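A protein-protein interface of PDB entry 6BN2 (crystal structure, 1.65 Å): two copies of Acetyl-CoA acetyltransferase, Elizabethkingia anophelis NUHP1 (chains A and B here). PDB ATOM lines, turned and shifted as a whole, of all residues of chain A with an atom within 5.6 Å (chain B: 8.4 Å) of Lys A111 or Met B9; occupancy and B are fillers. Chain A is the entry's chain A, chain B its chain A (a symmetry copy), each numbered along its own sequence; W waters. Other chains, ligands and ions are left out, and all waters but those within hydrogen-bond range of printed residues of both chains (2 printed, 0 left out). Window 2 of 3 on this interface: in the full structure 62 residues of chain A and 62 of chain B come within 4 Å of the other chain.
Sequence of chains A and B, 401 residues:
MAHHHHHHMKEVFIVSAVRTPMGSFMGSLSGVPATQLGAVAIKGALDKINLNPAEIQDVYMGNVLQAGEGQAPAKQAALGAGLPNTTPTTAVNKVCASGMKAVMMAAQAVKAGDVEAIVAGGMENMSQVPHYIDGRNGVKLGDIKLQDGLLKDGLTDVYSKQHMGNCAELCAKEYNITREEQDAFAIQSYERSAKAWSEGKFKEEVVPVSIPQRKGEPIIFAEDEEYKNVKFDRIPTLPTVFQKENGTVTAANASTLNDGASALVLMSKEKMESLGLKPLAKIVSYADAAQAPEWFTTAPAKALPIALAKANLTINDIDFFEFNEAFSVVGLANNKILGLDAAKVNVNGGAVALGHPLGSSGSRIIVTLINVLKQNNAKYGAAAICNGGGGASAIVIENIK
The side-chain carboxylate (OD2) of Asp B114 is in hydrogen-bond range of the side-chain amide nitrogen (NE2) of Gln A108 (2.8 Å). The side-chain carboxylate of Asp A114 is in hydrogen-bond range of the side-chain amide nitrogen of Gln B108 (2.8 Å). The side-chain hydroxyl (OH) of Tyr B286 sits at hydrogen-bond distance from the side-chain carboxylate (OD2) of Asp A114 (2.6 Å). OH of Tyr A286 is in hydrogen-bond range of OD2 of Asp B114. The backbone carbonyl oxygen (O) of Ala B112 lies close to the side-chain sulfur (SD) of Met A9, 3.7 Å away. The backbone carbonyl oxygen (O) of Ala A112 lies close to the side-chain sulfur (SD) of Met B9 (3.7 Å).
The backbone carbonyl oxygen (O) of Ala A109 sits at hydrogen-bond distance from the backbone NH (N) of Asp A114. OH of Tyr A286 lies within hydrogen-bond range of NZ of Lys A111 (3.0 Å). N of Asp B114 lies within hydrogen-bond range of O of Ala B109 (3.1 Å). The side-chain hydroxyl (OH) of Tyr B286 is in hydrogen-bond range of the side-chain amino group (NZ) of Lys B111 (3.0 Å).
O of Lys B111 touches SD of Met A9, at 3.8 Å. Ala B109 touches Gln A108. Gln A108 touches Ala B112. Ala A109 touches Gln B108. O of Lys A111 touches SD of Met B9, at 3.8 Å. CE of Lys A111 touches O of Ala B112, at 3.5 Å. Ala A112 touches Gln B108. Lys B111 touches Ala A112 (CE to O, 3.5 Å).
Met B9 touches just these residues of chain A: Lys A111 and Ala A112. Of the printed residues of chain B, Ala A112 touches Met B9 (3.4 Å), Gln B108 (3.96 Å) and Lys B111 (3.5 Å). Of the printed residues of chain A, Ala B109 touches Gln A108 (3.6 Å). Printed residues of chain A within 4 Å of Lys B111: Met A9 (3.8 Å) and Ala A112 (3.5 Å). Printed residues of chain A within 4 Å of Ala B112: Met A9 (3.4 Å), Gln A108 (3.96 Å) and Lys A111 (3.5 Å).
Printed residues of chain A that touch a printed residue of chain B: Met A9, Gln A108, Ala A109, Lys A111, Ala A112, Asp A114 and Tyr A286. Hydrophobic or aromatic side chains of chain A that line the printed part of chain B: Met A9, Ala A109, Ala A112 and Tyr A286. Hydrophobic or aromatic side chains of chain B that line the printed part of chain A: Met B9, Ala B109, Ala B112 and Tyr B286. Among the printed residues, 14 pairs touch across the chains. Among the printed residues, no Asp or Glu carboxylate lies within 4 Å of a Lys or Arg side-chain nitrogen of the other chain.
Met A9 touches Lys B111, and with the chains exchanged Lys A111 touches Met B9. Met A9 touches Ala B112, and with the chains exchanged Ala A112 touches Met B9. Gln A108 touches Ala B112, and with the chains exchanged Ala A112 touches Gln B108. Gln A108 touches Asp B114, and with the chains exchanged Asp A114 touches Gln B108. Positions printed for both chains: 9, 10, 11, 12, 107, 108, 109, 110, 111, 112, 113, 114 and 286.
Water W1 lies within hydrogen-bond range of NZ of Lys A111 (2.6 Å), OD1 of Asp B114 (2.7 Å) and O of Ala B112 (2.8 Å). Water W2 lies within hydrogen-bond range of NZ of Lys B111 (2.6 Å), OD1 of Asp A114 (2.7 Å) and O of Ala A112 (2.8 Å).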
ATOM      1  N   MET A   9      -0.735 -19.397  20.092  1.00  0.00           N
ATOM      2  CA  MET A   9      -1.329 -20.473  20.877  1.00  0.00           C
ATOM      3  C   MET A   9      -0.280 -21.114  21.796  1.00  0.00           C
ATOM      4  O   MET A   9       0.873 -21.280  21.392  1.00  0.00           O
ATOM      5  CB  MET A   9      -1.944 -21.533  19.954  1.00  0.00           C
ATOM      6  CG  MET A   9      -3.188 -22.220  20.509  1.00  0.00           C
ATOM      7  SD  MET A   9      -4.702 -21.240  20.362  1.00  0.00           S
ATOM      8  CE  MET A   9      -4.827 -21.047  18.584  1.00  0.00           C
ATOM      9  N   LYS A  10      -0.692 -21.462  23.023  1.00  0.00           N
ATOM     10  CA  LYS A  10       0.180 -22.138  23.978  1.00  0.00           C
ATOM     11  C   LYS A  10       0.782 -23.398  23.376  1.00  0.00           C
ATOM     12  O   LYS A  10       0.102 -24.166  22.692  1.00  0.00           O
ATOM     13  CB  LYS A  10      -0.601 -22.551  25.229  1.00  0.00           C
ATOM     14  CG  LYS A  10      -0.804 -21.503  26.277  1.00  0.00           C
ATOM     15  CD  LYS A  10      -1.349 -22.163  27.526  1.00  0.00           C
ATOM     16  CE  LYS A  10      -1.784 -21.135  28.542  1.00  0.00           C
ATOM     17  NZ  LYS A  10      -2.119 -21.779  29.836  1.00  0.00           N
ATOM     18  N   GLU A  11       2.045 -23.645  23.689  1.00  0.00           N
ATOM     19  CA  GLU A  11       2.643 -24.921  23.338  1.00  0.00           C
ATOM     20  C   GLU A  11       2.177 -26.011  24.296  1.00  0.00           C
ATOM     21  O   GLU A  11       1.810 -25.747  25.446  1.00  0.00           O
ATOM     22  CB  GLU A  11       4.170 -24.819  23.368  1.00  0.00           C
ATOM     23  CG  GLU A  11       4.745 -23.858  22.349  1.00  0.00           C
ATOM     24  CD  GLU A  11       6.218 -23.589  22.592  1.00  0.00           C
ATOM     25  OE1 GLU A  11       6.564 -23.119  23.699  1.00  0.00           O
ATOM     26  OE2 GLU A  11       7.028 -23.857  21.683  1.00  0.00           O
ATOM     27  N   VAL A  12       2.187 -27.249  23.809  1.00  0.00           N
ATOM     28  CA  VAL A  12       1.830 -28.414  24.606  1.00  0.00           C
ATOM     29  C   VAL A  12       2.977 -29.398  24.530  1.00  0.00           C
ATOM     30  O   VAL A  12       3.381 -29.795  23.431  1.00  0.00           O
ATOM     31  CB  VAL A  12       0.539 -29.085  24.108  1.00  0.00           C
ATOM     32  CG1 VAL A  12       0.121 -30.204  25.076  1.00  0.00           C
ATOM     33  CG2 VAL A  12      -0.549 -28.032  23.962  1.00  0.00           C
ATOM     34  N   ALA A 106      -6.828 -33.647  24.952  1.00  0.00           N
ATOM     35  CA  ALA A 106      -6.093 -33.118  26.092  1.00  0.00           C
ATOM     36  C   ALA A 106      -5.219 -31.939  25.679  1.00  0.00           C
ATOM     37  O   ALA A 106      -5.121 -30.940  26.405  1.00  0.00           O
ATOM     38  CB  ALA A 106      -5.254 -34.231  26.727  1.00  0.00           C
ATOM     39  N   ALA A 107      -4.577 -32.038  24.508  1.00  0.00           N
ATOM     40  CA  ALA A 107      -3.793 -30.916  24.010  1.00  0.00           C
ATOM     41  C   ALA A 107      -4.680 -29.695  23.787  1.00  0.00           C
ATOM     42  O   ALA A 107      -4.281 -28.556  24.085  1.00  0.00           O
ATOM     43  CB  ALA A 107      -3.061 -31.327  22.724  1.00  0.00           C
ATOM     44  N   GLN A 108      -5.901 -29.913  23.300  1.00  0.00           N
ATOM     45  CA  GLN A 108      -6.819 -28.800  23.098  1.00  0.00           C
ATOM     46  C   GLN A 108      -7.213 -28.164  24.421  1.00  0.00           C
ATOM     47  O   GLN A 108      -7.399 -26.947  24.485  1.00  0.00           O
ATOM     48  CB  GLN A 108      -8.059 -29.267  22.332  1.00  0.00           C
ATOM     49  CG  GLN A 108      -7.714 -29.633  20.882  1.00  0.00           C
ATOM     50  CD  GLN A 108      -8.841 -30.295  20.137  1.00  0.00           C
ATOM     51  OE1 GLN A 108      -9.509 -31.174  20.658  1.00  0.00           O
ATOM     52  NE2 GLN A 108      -9.072 -29.861  18.908  1.00  0.00           N
ATOM     53  N   ALA A 109      -7.351 -28.967  25.483  1.00  0.00           N
ATOM     54  CA  ALA A 109      -7.641 -28.401  26.804  1.00  0.00           C
ATOM     55  C   ALA A 109      -6.503 -27.506  27.288  1.00  0.00           C
ATOM     56  O   ALA A 109      -6.746 -26.473  27.934  1.00  0.00           O
ATOM     57  CB  ALA A 109      -7.902 -29.521  27.818  1.00  0.00           C
ATOM     58  N   VAL A 110      -5.254 -27.879  26.986  1.00  0.00           N
ATOM     59  CA  VAL A 110      -4.120 -27.013  27.327  1.00  0.00           C
ATOM     60  C   VAL A 110      -4.137 -25.747  26.469  1.00  0.00           C
ATOM     61  O   VAL A 110      -3.991 -24.628  26.981  1.00  0.00           O
ATOM     62  CB  VAL A 110      -2.782 -27.767  27.180  1.00  0.00           C
ATOM     63  CG1 VAL A 110      -1.582 -26.822  27.481  1.00  0.00           C
ATOM     64  CG2 VAL A 110      -2.727 -28.973  28.121  1.00  0.00           C
ATOM     65  N   LYS A 111      -4.313 -25.904  25.152  1.00  0.00           N
ATOM     66  CA  LYS A 111      -4.292 -24.740  24.263  1.00  0.00           C
ATOM     67  C   LYS A 111      -5.442 -23.782  24.546  1.00  0.00           C
ATOM     68  O   LYS A 111      -5.295 -22.563  24.357  1.00  0.00           O
ATOM     69  CB  LYS A 111      -4.324 -25.202  22.801  1.00  0.00           C
ATOM     70  CG  LYS A 111      -3.048 -25.892  22.383  1.00  0.00           C
ATOM     71  CD  LYS A 111      -3.175 -26.645  21.072  1.00  0.00           C
ATOM     72  CE  LYS A 111      -3.325 -25.728  19.883  1.00  0.00           C
ATOM     73  NZ  LYS A 111      -3.196 -26.538  18.619  1.00  0.00           N
ATOM     74  N   ALA A 112      -6.586 -24.306  24.987  1.00  0.00           N
ATOM     75  CA  ALA A 112      -7.746 -23.481  25.298  1.00  0.00           C
ATOM     76  C   ALA A 112      -7.586 -22.727  26.604  1.00  0.00           C
ATOM     77  O   ALA A 112      -8.460 -21.920  26.939  1.00  0.00           O
ATOM     78  CB  ALA A 112      -9.010 -24.344  25.354  1.00  0.00           C
ATOM     79  N   GLY A 113      -6.512 -22.987  27.344  1.00  0.00           N
ATOM     80  CA  GLY A 113      -6.210 -22.293  28.576  1.00  0.00           C
ATOM     81  C   GLY A 113      -6.789 -22.912  29.826  1.00  0.00           C
ATOM     82  O   GLY A 113      -6.656 -22.322  30.905  1.00  0.00           O
ATOM     83  N   ASP A 114      -7.399 -24.091  29.726  1.00  0.00           N
ATOM     84  CA  ASP A 114      -8.201 -24.600  30.830  1.00  0.00           C
ATOM     85  C   ASP A 114      -7.420 -25.461  31.804  1.00  0.00           C
ATOM     86  O   ASP A 114      -7.791 -25.525  32.985  1.00  0.00           O
ATOM     87  CB  ASP A 114      -9.381 -25.408  30.297  1.00  0.00           C
ATOM     88  CG  ASP A 114     -10.369 -24.543  29.578  1.00  0.00           C
ATOM     89  OD1 ASP A 114     -10.776 -23.526  30.173  1.00  0.00           O
ATOM     90  OD2 ASP A 114     -10.717 -24.877  28.426  1.00  0.00           O
ATOM     91  N   VAL A 284       3.232 -30.842  17.894  1.00  0.00           N
ATOM     92  CA  VAL A 284       3.286 -29.775  16.897  1.00  0.00           C
ATOM     93  C   VAL A 284       1.903 -29.493  16.318  1.00  0.00           C
ATOM     94  O   VAL A 284       1.487 -28.331  16.226  1.00  0.00           O
ATOM     95  CB  VAL A 284       4.285 -30.139  15.787  1.00  0.00           C
ATOM     96  CG1 VAL A 284       4.296 -29.060  14.715  1.00  0.00           C
ATOM     97  CG2 VAL A 284       5.688 -30.340  16.373  1.00  0.00           C
ATOM     98  N   TYR A 286      -2.070 -31.809  14.962  1.00  0.00           N
ATOM     99  CA  TYR A 286      -2.843 -33.046  14.941  1.00  0.00           C
ATOM    100  C   TYR A 286      -4.068 -32.793  14.080  1.00  0.00           C
ATOM    101  O   TYR A 286      -4.428 -31.642  13.811  1.00  0.00           O
ATOM    102  CB  TYR A 286      -3.256 -33.514  16.362  1.00  0.00           C
ATOM    103  CG  TYR A 286      -3.720 -32.338  17.174  1.00  0.00           C
ATOM    104  CD1 TYR A 286      -5.013 -31.845  17.025  1.00  0.00           C
ATOM    105  CD2 TYR A 286      -2.850 -31.666  18.021  1.00  0.00           C
ATOM    106  CE1 TYR A 286      -5.426 -30.715  17.698  1.00  0.00           C
ATOM    107  CE2 TYR A 286      -3.257 -30.534  18.707  1.00  0.00           C
ATOM    108  CZ  TYR A 286      -4.543 -30.068  18.538  1.00  0.00           C
ATOM    109  OH  TYR A 286      -4.961 -28.921  19.186  1.00  0.00           O
ATOM    110  N   MET B   9      -8.571 -15.203  23.914  1.00  0.00           N
ATOM    111  CA  MET B   9      -9.085 -16.486  23.448  1.00  0.00           C
ATOM    112  C   MET B   9     -10.340 -16.286  22.589  1.00  0.00           C
ATOM    113  O   MET B   9     -11.167 -15.427  22.899  1.00  0.00           O
ATOM    114  CB  MET B   9      -9.396 -17.402  24.639  1.00  0.00           C
ATOM    115  CG  MET B   9      -9.172 -18.889  24.378  1.00  0.00           C
ATOM    116  SD  MET B   9      -7.439 -19.402  24.462  1.00  0.00           S
ATOM    117  CE  MET B   9      -7.030 -18.989  26.158  1.00  0.00           C
ATOM    118  N   LYS B  10     -10.464 -17.081  21.517  1.00  0.00           N
ATOM    119  CA  LYS B  10     -11.637 -17.045  20.648  1.00  0.00           C
ATOM    120  C   LYS B  10     -12.918 -17.231  21.446  1.00  0.00           C
ATOM    121  O   LYS B  10     -12.991 -18.070  22.347  1.00  0.00           O
ATOM    122  CB  LYS B  10     -11.573 -18.164  19.604  1.00  0.00           C
ATOM    123  CG  LYS B  10     -10.756 -17.901  18.379  1.00  0.00           C
ATOM    124  CD  LYS B  10     -11.033 -18.993  17.367  1.00  0.00           C
ATOM    125  CE  LYS B  10     -10.078 -18.913  16.202  1.00  0.00           C
ATOM    126  NZ  LYS B  10     -10.483 -19.845  15.120  1.00  0.00           N
ATOM    127  N   GLU B  11     -13.950 -16.496  21.066  1.00  0.00           N
ATOM    128  CA  GLU B  11     -15.266 -16.750  21.625  1.00  0.00           C
ATOM    129  C   GLU B  11     -15.890 -17.983  20.981  1.00  0.00           C
ATOM    130  O   GLU B  11     -15.571 -18.350  19.845  1.00  0.00           O
ATOM    131  CB  GLU B  11     -16.177 -15.537  21.417  1.00  0.00           C
ATOM    132  CG  GLU B  11     -15.714 -14.288  22.137  1.00  0.00           C
ATOM    133  CD  GLU B  11     -16.485 -13.059  21.691  1.00  0.00           C
ATOM    134  OE1 GLU B  11     -16.465 -12.750  20.479  1.00  0.00           O
ATOM    135  OE2 GLU B  11     -17.116 -12.411  22.549  1.00  0.00           O
ATOM    136  N   VAL B  12     -16.785 -18.630  21.723  1.00  0.00           N
ATOM    137  CA  VAL B  12     -17.519 -19.791  21.241  1.00  0.00           C
ATOM    138  C   VAL B  12     -18.996 -19.510  21.412  1.00  0.00           C
ATOM    139  O   VAL B  12     -19.445 -19.208  22.523  1.00  0.00           O
ATOM    140  CB  VAL B  12     -17.145 -21.073  22.003  1.00  0.00           C
ATOM    141  CG1 VAL B  12     -17.823 -22.289  21.350  1.00  0.00           C
ATOM    142  CG2 VAL B  12     -15.631 -21.217  22.025  1.00  0.00           C
ATOM    143  N   ALA B 107     -16.126 -26.853  22.784  1.00  0.00           N
ATOM    144  CA  ALA B 107     -15.730 -25.460  22.942  1.00  0.00           C
ATOM    145  C   ALA B 107     -14.210 -25.332  22.982  1.00  0.00           C
ATOM    146  O   ALA B 107     -13.635 -24.395  22.404  1.00  0.00           O
ATOM    147  CB  ALA B 107     -16.382 -24.877  24.205  1.00  0.00           C
ATOM    148  N   GLN B 108     -13.538 -26.286  23.628  1.00  0.00           N
ATOM    149  CA  GLN B 108     -12.083 -26.252  23.675  1.00  0.00           C
ATOM    150  C   GLN B 108     -11.483 -26.448  22.293  1.00  0.00           C
ATOM    151  O   GLN B 108     -10.447 -25.855  21.984  1.00  0.00           O
ATOM    152  CB  GLN B 108     -11.559 -27.311  24.647  1.00  0.00           C
ATOM    153  CG  GLN B 108     -11.910 -26.958  26.099  1.00  0.00           C
ATOM    154  CD  GLN B 108     -11.609 -28.057  27.082  1.00  0.00           C
ATOM    155  OE1 GLN B 108     -11.898 -29.217  26.838  1.00  0.00           O
ATOM    156  NE2 GLN B 108     -11.005 -27.697  28.204  1.00  0.00           N
ATOM    157  N   ALA B 109     -12.111 -27.279  21.452  1.00  0.00           N
ATOM    158  CA  ALA B 109     -11.631 -27.440  20.076  1.00  0.00           C
ATOM    159  C   ALA B 109     -11.736 -26.132  19.294  1.00  0.00           C
ATOM    160  O   ALA B 109     -10.862 -25.823  18.466  1.00  0.00           O
ATOM    161  CB  ALA B 109     -12.415 -28.547  19.363  1.00  0.00           C
ATOM    162  N   VAL B 110     -12.792 -25.349  19.540  1.00  0.00           N
ATOM    163  CA  VAL B 110     -12.902 -24.033  18.904  1.00  0.00           C
ATOM    164  C   VAL B 110     -11.844 -23.079  19.462  1.00  0.00           C
ATOM    165  O   VAL B 110     -11.143 -22.392  18.706  1.00  0.00           O
ATOM    166  CB  VAL B 110     -14.321 -23.450  19.074  1.00  0.00           C
ATOM    167  CG1 VAL B 110     -14.409 -22.025  18.452  1.00  0.00           C
ATOM    168  CG2 VAL B 110     -15.367 -24.355  18.419  1.00  0.00           C
ATOM    169  N   LYS B 111     -11.714 -23.022  20.792  1.00  0.00           N
ATOM    170  CA  LYS B 111     -10.755 -22.095  21.399  1.00  0.00           C
ATOM    171  C   LYS B 111      -9.317 -22.439  21.032  1.00  0.00           C
ATOM    172  O   LYS B 111      -8.468 -21.537  20.934  1.00  0.00           O
ATOM    173  CB  LYS B 111     -10.935 -22.084  22.922  1.00  0.00           C
ATOM    174  CG  LYS B 111     -12.237 -21.450  23.347  1.00  0.00           C
ATOM    175  CD  LYS B 111     -12.591 -21.724  24.797  1.00  0.00           C
ATOM    176  CE  LYS B 111     -11.678 -21.014  25.765  1.00  0.00           C
ATOM    177  NZ  LYS B 111     -12.245 -21.138  27.156  1.00  0.00           N
ATOM    178  N   ALA B 112      -9.021 -23.725  20.836  1.00  0.00           N
ATOM    179  CA  ALA B 112      -7.681 -24.165  20.473  1.00  0.00           C
ATOM    180  C   ALA B 112      -7.346 -23.864  19.024  1.00  0.00           C
ATOM    181  O   ALA B 112      -6.206 -24.103  18.613  1.00  0.00           O
ATOM    182  CB  ALA B 112      -7.526 -25.665  20.737  1.00  0.00           C
ATOM    183  N   GLY B 113      -8.311 -23.372  18.253  1.00  0.00           N
ATOM    184  CA  GLY B 113      -8.106 -22.986  16.875  1.00  0.00           C
ATOM    185  C   GLY B 113      -8.331 -24.078  15.857  1.00  0.00           C
ATOM    186  O   GLY B 113      -8.080 -23.850  14.667  1.00  0.00           O
ATOM    187  N   ASP B 114      -8.820 -25.244  16.274  1.00  0.00           N
ATOM    188  CA  ASP B 114      -8.802 -26.405  15.395  1.00  0.00           C
ATOM    189  C   ASP B 114     -10.058 -26.556  14.558  1.00  0.00           C
ATOM    190  O   ASP B 114      -9.989 -27.135  13.465  1.00  0.00           O
ATOM    191  CB  ASP B 114      -8.600 -27.680  16.210  1.00  0.00           C
ATOM    192  CG  ASP B 114      -7.234 -27.740  16.820  1.00  0.00           C
ATOM    193  OD1 ASP B 114      -6.262 -27.553  16.063  1.00  0.00           O
ATOM    194  OD2 ASP B 114      -7.144 -27.957  18.047  1.00  0.00           O
ATOM    195  N   LYS B 282     -23.758 -17.277  24.104  1.00  0.00           N
ATOM    196  CA  LYS B 282     -22.302 -17.377  24.103  1.00  0.00           C
ATOM    197  C   LYS B 282     -21.886 -18.266  25.263  1.00  0.00           C
ATOM    198  O   LYS B 282     -22.464 -18.180  26.346  1.00  0.00           O
ATOM    199  CB  LYS B 282     -21.677 -15.977  24.246  1.00  0.00           C
ATOM    200  CG  LYS B 282     -20.167 -15.970  24.404  1.00  0.00           C
ATOM    201  CD  LYS B 282     -19.672 -14.520  24.423  1.00  0.00           C
ATOM    202  CE  LYS B 282     -18.381 -14.374  25.208  1.00  0.00           C
ATOM    203  NZ  LYS B 282     -17.878 -12.963  25.151  1.00  0.00           N
ATOM    204  N   TYR B 286     -16.590 -22.727  31.741  1.00  0.00           N
ATOM    205  CA  TYR B 286     -17.027 -24.069  32.111  1.00  0.00           C
ATOM    206  C   TYR B 286     -15.957 -24.653  33.017  1.00  0.00           C
ATOM    207  O   TYR B 286     -14.825 -24.160  33.063  1.00  0.00           O
ATOM    208  CB  TYR B 286     -17.261 -24.980  30.876  1.00  0.00           C
ATOM    209  CG  TYR B 286     -16.154 -24.785  29.879  1.00  0.00           C
ATOM    210  CD1 TYR B 286     -14.932 -25.430  30.048  1.00  0.00           C
ATOM    211  CD2 TYR B 286     -16.292 -23.898  28.821  1.00  0.00           C
ATOM    212  CE1 TYR B 286     -13.878 -25.194  29.191  1.00  0.00           C
ATOM    213  CE2 TYR B 286     -15.243 -23.660  27.950  1.00  0.00           C
ATOM    214  CZ  TYR B 286     -14.043 -24.312  28.144  1.00  0.00           C
ATOM    215  OH  TYR B 286     -12.971 -24.064  27.307  1.00  0.00           O
HETATM  216  O   HOH W   1      -4.649 -25.469  16.784  1.00  0.00           O
HETATM  217  O   HOH W   2     -10.310 -21.180  28.853  1.00  0.00           O
